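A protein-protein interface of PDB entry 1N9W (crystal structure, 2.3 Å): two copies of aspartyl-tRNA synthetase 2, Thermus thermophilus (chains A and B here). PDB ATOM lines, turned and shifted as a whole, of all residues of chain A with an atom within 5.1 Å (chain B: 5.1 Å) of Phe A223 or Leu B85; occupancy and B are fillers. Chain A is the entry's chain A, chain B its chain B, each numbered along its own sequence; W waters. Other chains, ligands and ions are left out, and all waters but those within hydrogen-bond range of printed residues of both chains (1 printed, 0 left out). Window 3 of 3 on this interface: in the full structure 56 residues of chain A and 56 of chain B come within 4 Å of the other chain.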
ATOM      1  N   GLU A 191      11.699   4.651   3.937  1.00  0.00           N
ATOM      2  CA  GLU A 191      12.948   3.884   4.092  1.00  0.00           C
ATOM      3  C   GLU A 191      13.615   3.916   5.467  1.00  0.00           C
ATOM      4  O   GLU A 191      14.161   2.910   5.916  1.00  0.00           O
ATOM      5  CB  GLU A 191      13.963   4.313   3.028  1.00  0.00           C
ATOM      6  CG  GLU A 191      13.659   3.760   1.647  1.00  0.00           C
ATOM      7  CD  GLU A 191      14.510   4.380   0.548  1.00  0.00           C
ATOM      8  OE1 GLU A 191      15.674   4.733   0.824  1.00  0.00           O
ATOM      9  OE2 GLU A 191      14.001   4.489  -0.586  1.00  0.00           O
ATOM     10  N   MET A 221      14.523   1.263  10.257  1.00  0.00           N
ATOM     11  CA  MET A 221      15.152   1.461   8.965  1.00  0.00           C
ATOM     12  C   MET A 221      15.158   0.219   8.072  1.00  0.00           C
ATOM     13  O   MET A 221      15.272  -0.915   8.550  1.00  0.00           O
ATOM     14  CB  MET A 221      16.584   1.991   9.156  1.00  0.00           C
ATOM     15  CG  MET A 221      17.580   1.041   9.836  1.00  0.00           C
ATOM     16  SD  MET A 221      19.193   1.820  10.346  1.00  0.00           S
ATOM     17  CE  MET A 221      19.866   2.336   8.753  1.00  0.00           C
ATOM     18  N   GLY A 222      15.017   0.462   6.767  1.00  0.00           N
ATOM     19  CA  GLY A 222      15.006  -0.606   5.783  1.00  0.00           C
ATOM     20  C   GLY A 222      16.258  -0.650   4.929  1.00  0.00           C
ATOM     21  O   GLY A 222      17.087   0.254   4.988  1.00  0.00           O
ATOM     22  N   PHE A 223      16.384  -1.699   4.119  1.00  0.00           N
ATOM     23  CA  PHE A 223      17.536  -1.916   3.229  1.00  0.00           C
ATOM     24  C   PHE A 223      18.828  -2.126   4.013  1.00  0.00           C
ATOM     25  O   PHE A 223      19.897  -1.651   3.618  1.00  0.00           O
ATOM     26  CB  PHE A 223      17.696  -0.757   2.239  1.00  0.00           C
ATOM     27  CG  PHE A 223      16.572  -0.675   1.239  1.00  0.00           C
ATOM     28  CD1 PHE A 223      16.447  -1.622   0.230  1.00  0.00           C
ATOM     29  CD2 PHE A 223      15.603   0.316   1.347  1.00  0.00           C
ATOM     30  CE1 PHE A 223      15.373  -1.591  -0.655  1.00  0.00           C
ATOM     31  CE2 PHE A 223      14.521   0.360   0.470  1.00  0.00           C
ATOM     32  CZ  PHE A 223      14.409  -0.600  -0.537  1.00  0.00           C
ATOM     33  N   ILE A 224      18.730  -2.845   5.131  1.00  0.00           N
ATOM     34  CA  ILE A 224      19.902  -3.126   5.953  1.00  0.00           C
ATOM     35  C   ILE A 224      20.457  -4.491   5.602  1.00  0.00           C
ATOM     36  O   ILE A 224      19.805  -5.288   4.929  1.00  0.00           O
ATOM     37  CB  ILE A 224      19.571  -3.153   7.452  1.00  0.00           C
ATOM     38  CG1 ILE A 224      18.589  -4.302   7.746  1.00  0.00           C
ATOM     39  CG2 ILE A 224      19.042  -1.777   7.901  1.00  0.00           C
ATOM     40  CD1 ILE A 224      18.216  -4.455   9.213  1.00  0.00           C
ATOM     41  N   ALA A 225      21.662  -4.760   6.072  1.00  0.00           N
ATOM     42  CA  ALA A 225      22.303  -6.042   5.827  1.00  0.00           C
ATOM     43  C   ALA A 225      21.876  -7.046   6.898  1.00  0.00           C
ATOM     44  O   ALA A 225      21.554  -8.195   6.591  1.00  0.00           O
ATOM     45  CB  ALA A 225      23.838  -5.867   5.827  1.00  0.00           C
ATOM     46  N   ASP A 229      23.667  -3.514  11.402  1.00  0.00           N
ATOM     47  CA  ASP A 229      23.482  -2.159  10.885  1.00  0.00           C
ATOM     48  C   ASP A 229      22.738  -1.339  11.950  1.00  0.00           C
ATOM     49  O   ASP A 229      22.968  -0.139  12.108  1.00  0.00           O
ATOM     50  CB  ASP A 229      22.642  -2.165   9.594  1.00  0.00           C
ATOM     51  CG  ASP A 229      23.387  -2.712   8.391  1.00  0.00           C
ATOM     52  OD1 ASP A 229      24.447  -3.352   8.560  1.00  0.00           O
ATOM     53  OD2 ASP A 229      22.894  -2.502   7.260  1.00  0.00           O
ATOM     54  N   HIS A 354      10.770  -9.918   6.985  1.00  0.00           N
ATOM     55  CA  HIS A 354      10.185  -9.131   5.900  1.00  0.00           C
ATOM     56  C   HIS A 354       9.500  -9.986   4.845  1.00  0.00           C
ATOM     57  O   HIS A 354       8.798  -9.457   3.972  1.00  0.00           O
ATOM     58  CB  HIS A 354      11.251  -8.236   5.247  1.00  0.00           C
ATOM     59  CG  HIS A 354      12.426  -8.991   4.712  1.00  0.00           C
ATOM     60  ND1 HIS A 354      12.496  -9.427   3.405  1.00  0.00           N
ATOM     61  CD2 HIS A 354      13.545  -9.441   5.326  1.00  0.00           C
ATOM     62  CE1 HIS A 354      13.613 -10.120   3.241  1.00  0.00           C
ATOM     63  NE2 HIS A 354      14.264 -10.143   4.390  1.00  0.00           N
ATOM     64  N   PRO A 385      11.334  -4.446   2.354  1.00  0.00           N
ATOM     65  CA  PRO A 385      12.755  -4.767   2.276  1.00  0.00           C
ATOM     66  C   PRO A 385      13.288  -5.242   3.632  1.00  0.00           C
ATOM     67  O   PRO A 385      12.623  -5.094   4.651  1.00  0.00           O
ATOM     68  CB  PRO A 385      13.362  -3.432   1.894  1.00  0.00           C
ATOM     69  CG  PRO A 385      12.548  -2.488   2.758  1.00  0.00           C
ATOM     70  CD  PRO A 385      11.124  -2.994   2.510  1.00  0.00           C
ATOM     71  N   PRO A 386      14.495  -5.832   3.648  1.00  0.00           N
ATOM     72  CA  PRO A 386      15.081  -6.286   4.910  1.00  0.00           C
ATOM     73  C   PRO A 386      15.045  -5.021   5.758  1.00  0.00           C
ATOM     74  O   PRO A 386      15.421  -3.947   5.285  1.00  0.00           O
ATOM     75  CB  PRO A 386      16.511  -6.649   4.517  1.00  0.00           C
ATOM     76  CG  PRO A 386      16.344  -7.162   3.132  1.00  0.00           C
ATOM     77  CD  PRO A 386      15.366  -6.165   2.512  1.00  0.00           C
ATOM     78  N   HIS A 387      14.588  -5.129   6.998  1.00  0.00           N
ATOM     79  CA  HIS A 387      14.460  -3.951   7.840  1.00  0.00           C
ATOM     80  C   HIS A 387      14.488  -4.313   9.300  1.00  0.00           C
ATOM     81  O   HIS A 387      14.295  -5.466   9.676  1.00  0.00           O
ATOM     82  CB  HIS A 387      13.136  -3.239   7.531  1.00  0.00           C
ATOM     83  CG  HIS A 387      11.920  -4.076   7.808  1.00  0.00           C
ATOM     84  ND1 HIS A 387      11.168  -3.947   8.957  1.00  0.00           N
ATOM     85  CD2 HIS A 387      11.346  -5.070   7.096  1.00  0.00           C
ATOM     86  CE1 HIS A 387      10.183  -4.824   8.939  1.00  0.00           C
ATOM     87  NE2 HIS A 387      10.266  -5.521   7.821  1.00  0.00           N
ATOM     88  N   LEU B  19      18.868   1.536  -4.595  1.00  0.00           N
ATOM     89  CA  LEU B  19      18.058   0.698  -3.707  1.00  0.00           C
ATOM     90  C   LEU B  19      16.692   1.363  -3.739  1.00  0.00           C
ATOM     91  O   LEU B  19      16.597   2.585  -3.631  1.00  0.00           O
ATOM     92  CB  LEU B  19      18.598   0.688  -2.270  1.00  0.00           C
ATOM     93  CG  LEU B  19      20.002   0.076  -2.081  1.00  0.00           C
ATOM     94  CD1 LEU B  19      20.450   0.232  -0.626  1.00  0.00           C
ATOM     95  CD2 LEU B  19      19.970  -1.396  -2.490  1.00  0.00           C
ATOM     96  N   GLY B  20      15.638   0.575  -3.928  1.00  0.00           N
ATOM     97  CA  GLY B  20      14.300   1.150  -3.972  1.00  0.00           C
ATOM     98  C   GLY B  20      13.232   0.118  -4.276  1.00  0.00           C
ATOM     99  O   GLY B  20      13.444  -1.074  -4.061  1.00  0.00           O
ATOM    100  N   PHE B  21      12.083   0.574  -4.762  1.00  0.00           N
ATOM    101  CA  PHE B  21      10.975  -0.324  -5.096  1.00  0.00           C
ATOM    102  C   PHE B  21      10.565  -0.177  -6.546  1.00  0.00           C
ATOM    103  O   PHE B  21      10.590   0.925  -7.094  1.00  0.00           O
ATOM    104  CB  PHE B  21       9.747  -0.031  -4.232  1.00  0.00           C
ATOM    105  CG  PHE B  21       9.999  -0.137  -2.762  1.00  0.00           C
ATOM    106  CD1 PHE B  21      10.547   0.933  -2.057  1.00  0.00           C
ATOM    107  CD2 PHE B  21       9.710  -1.316  -2.081  1.00  0.00           C
ATOM    108  CE1 PHE B  21      10.792   0.830  -0.699  1.00  0.00           C
ATOM    109  CE2 PHE B  21       9.957  -1.425  -0.720  1.00  0.00           C
ATOM    110  CZ  PHE B  21      10.500  -0.355  -0.021  1.00  0.00           C
ATOM    111  N   ALA B  58      11.053  -4.945  -3.672  1.00  0.00           N
ATOM    112  CA  ALA B  58      12.207  -4.163  -3.239  1.00  0.00           C
ATOM    113  C   ALA B  58      13.377  -4.637  -4.090  1.00  0.00           C
ATOM    114  O   ALA B  58      13.606  -5.840  -4.226  1.00  0.00           O
ATOM    115  CB  ALA B  58      12.486  -4.399  -1.762  1.00  0.00           C
ATOM    116  N   LEU B  59      14.117  -3.692  -4.659  1.00  0.00           N
ATOM    117  CA  LEU B  59      15.235  -4.032  -5.532  1.00  0.00           C
ATOM    118  C   LEU B  59      16.547  -3.316  -5.261  1.00  0.00           C
ATOM    119  O   LEU B  59      16.611  -2.272  -4.607  1.00  0.00           O
ATOM    120  CB  LEU B  59      14.874  -3.704  -6.979  1.00  0.00           C
ATOM    121  CG  LEU B  59      13.573  -4.127  -7.631  1.00  0.00           C
ATOM    122  CD1 LEU B  59      13.542  -3.504  -9.012  1.00  0.00           C
ATOM    123  CD2 LEU B  59      13.467  -5.635  -7.708  1.00  0.00           C
ATOM    124  N   ARG B  60      17.596  -3.895  -5.819  1.00  0.00           N
ATOM    125  CA  ARG B  60      18.912  -3.305  -5.769  1.00  0.00           C
ATOM    126  C   ARG B  60      19.314  -3.303  -7.241  1.00  0.00           C
ATOM    127  O   ARG B  60      19.142  -4.313  -7.929  1.00  0.00           O
ATOM    128  CB  ARG B  60      19.872  -4.171  -4.956  1.00  0.00           C
ATOM    129  CG  ARG B  60      21.313  -3.748  -5.083  1.00  0.00           C
ATOM    130  CD  ARG B  60      22.189  -4.462  -4.078  1.00  0.00           C
ATOM    131  NE  ARG B  60      23.560  -4.474  -4.538  1.00  0.00           N
ATOM    132  CZ  ARG B  60      24.019  -5.266  -5.502  1.00  0.00           C
ATOM    133  NH1 ARG B  60      23.215  -6.131  -6.104  1.00  0.00           N
ATOM    134  NH2 ARG B  60      25.287  -5.169  -5.894  1.00  0.00           N
ATOM    135  N   GLU B  83      18.982  -7.148  -8.676  1.00  0.00           N
ATOM    136  CA  GLU B  83      18.762  -8.112  -7.593  1.00  0.00           C
ATOM    137  C   GLU B  83      17.437  -7.775  -6.907  1.00  0.00           C
ATOM    138  O   GLU B  83      17.203  -6.629  -6.526  1.00  0.00           O
ATOM    139  CB  GLU B  83      19.906  -8.049  -6.558  1.00  0.00           C
ATOM    140  CG  GLU B  83      19.695  -8.995  -5.358  1.00  0.00           C
ATOM    141  CD  GLU B  83      20.781  -8.914  -4.272  1.00  0.00           C
ATOM    142  OE1 GLU B  83      20.713  -9.708  -3.308  1.00  0.00           O
ATOM    143  OE2 GLU B  83      21.695  -8.074  -4.365  1.00  0.00           O
ATOM    144  N   VAL B  84      16.574  -8.776  -6.769  1.00  0.00           N
ATOM    145  CA  VAL B  84      15.292  -8.580  -6.112  1.00  0.00           C
ATOM    146  C   VAL B  84      15.522  -8.887  -4.640  1.00  0.00           C
ATOM    147  O   VAL B  84      15.790 -10.027  -4.281  1.00  0.00           O
ATOM    148  CB  VAL B  84      14.221  -9.537  -6.683  1.00  0.00           C
ATOM    149  CG1 VAL B  84      12.834  -9.161  -6.167  1.00  0.00           C
ATOM    150  CG2 VAL B  84      14.251  -9.485  -8.200  1.00  0.00           C
ATOM    151  N   LEU B  85      15.449  -7.859  -3.799  1.00  0.00           N
ATOM    152  CA  LEU B  85      15.672  -8.018  -2.364  1.00  0.00           C
ATOM    153  C   LEU B  85      14.448  -8.598  -1.662  1.00  0.00           C
ATOM    154  O   LEU B  85      14.569  -9.317  -0.671  1.00  0.00           O
ATOM    155  CB  LEU B  85      16.017  -6.657  -1.748  1.00  0.00           C
ATOM    156  CG  LEU B  85      17.225  -5.970  -2.390  1.00  0.00           C
ATOM    157  CD1 LEU B  85      17.365  -4.543  -1.873  1.00  0.00           C
ATOM    158  CD2 LEU B  85      18.483  -6.799  -2.079  1.00  0.00           C
ATOM    159  N   SER B  86      13.271  -8.277  -2.186  1.00  0.00           N
ATOM    160  CA  SER B  86      12.028  -8.751  -1.602  1.00  0.00           C
ATOM    161  C   SER B  86      10.922  -8.648  -2.636  1.00  0.00           C
ATOM    162  O   SER B  86      10.361  -7.578  -2.854  1.00  0.00           O
ATOM    163  CB  SER B  86      11.669  -7.900  -0.383  1.00  0.00           C
ATOM    164  OG  SER B  86      10.468  -8.325   0.205  1.00  0.00           O
ATOM    165  N   PRO B  87      10.599  -9.766  -3.300  1.00  0.00           N
ATOM    166  CA  PRO B  87       9.546  -9.788  -4.319  1.00  0.00           C
ATOM    167  C   PRO B  87       8.140  -9.635  -3.750  1.00  0.00           C
ATOM    168  O   PRO B  87       7.798 -10.231  -2.724  1.00  0.00           O
ATOM    169  CB  PRO B  87       9.743 -11.147  -4.994  1.00  0.00           C
ATOM    170  CG  PRO B  87      10.253 -12.004  -3.875  1.00  0.00           C
ATOM    171  CD  PRO B  87      11.246 -11.090  -3.177  1.00  0.00           C
HETATM  172  O   HOH W   1       7.510  -8.429   1.907  1.00  0.00           O
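The backbone NH of Phe A223 is in hydrogen-bond range of the backbone carbonyl oxygen of Pro A386 (2.7 Å).
O of Gly B20 sits at hydrogen-bond distance from N of Leu B59 (2.8 Å).
The backbone NH of Leu B85 sits at hydrogen-bond distance from the backbone carbonyl oxygen of Ala B58.
N of Ala B58 is in hydrogen-bond range of O of Ser B86 (2.8 Å).
Phe A223 touches Gly B20.
Phe A223 touches Phe B21.
CD1 of Leu B85 touches CD1 of Phe A223, at 3.7 Å.
His A354 touches Ser B86.
Pro A385 touches Phe B21 (CD to CZ, 3.7 Å).
CB of Pro A385 touches CB of Ala B58, 3.9 Å away.
Of the printed residues of chain B, Phe A223 touches Gly B20, Phe B21 and Leu B85.
Leu B85 touches one residue of chain A.
Of the printed residues of chain A, Ser B86 touches His A354 (3.9 Å).
Printed residues of chain B within 4 Å of Pro A385: Phe B21 and Ala B58.
Of the printed residues of chain B, His A354 touches Ser B86.
Printed residues of chain A within 4 Å of Ala B58: Pro A385.
Of the printed residues of chain A, Gly B20 touches Phe A223 (3.7 Å).
Ala A225 touches none of the printed residues of chain B.
The nearest printed residue of chain B that does not touch His A354 is Leu B85 (4.1 Å).
Of the 11 printed residues of chain B, 5 touch a printed residue of chain A.
Printed residues of chain B that touch a printed residue of chain A: Gly B20, Phe B21, Ala B58, Leu B85 and Ser B86.
Hydrophobic or aromatic side chains of chain B within 4 Å of the printed part of chain A: Phe B21, Ala B58 and Leu B85.
Hydrophobic or aromatic side chains of chain A that line the printed part of chain B: Phe A223, His A354 and Pro A385.
Among the printed residues, 6 pairs touch across the chains.
No position is printed for both chains.
Of the 6 pairs that touch across the chains among the printed residues, none has its exchanged pair printed and touching as well.
Water W1 lies within hydrogen-bond range of O of His A354 (2.6 Å) and OG of Ser B86 (3.4 Å).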
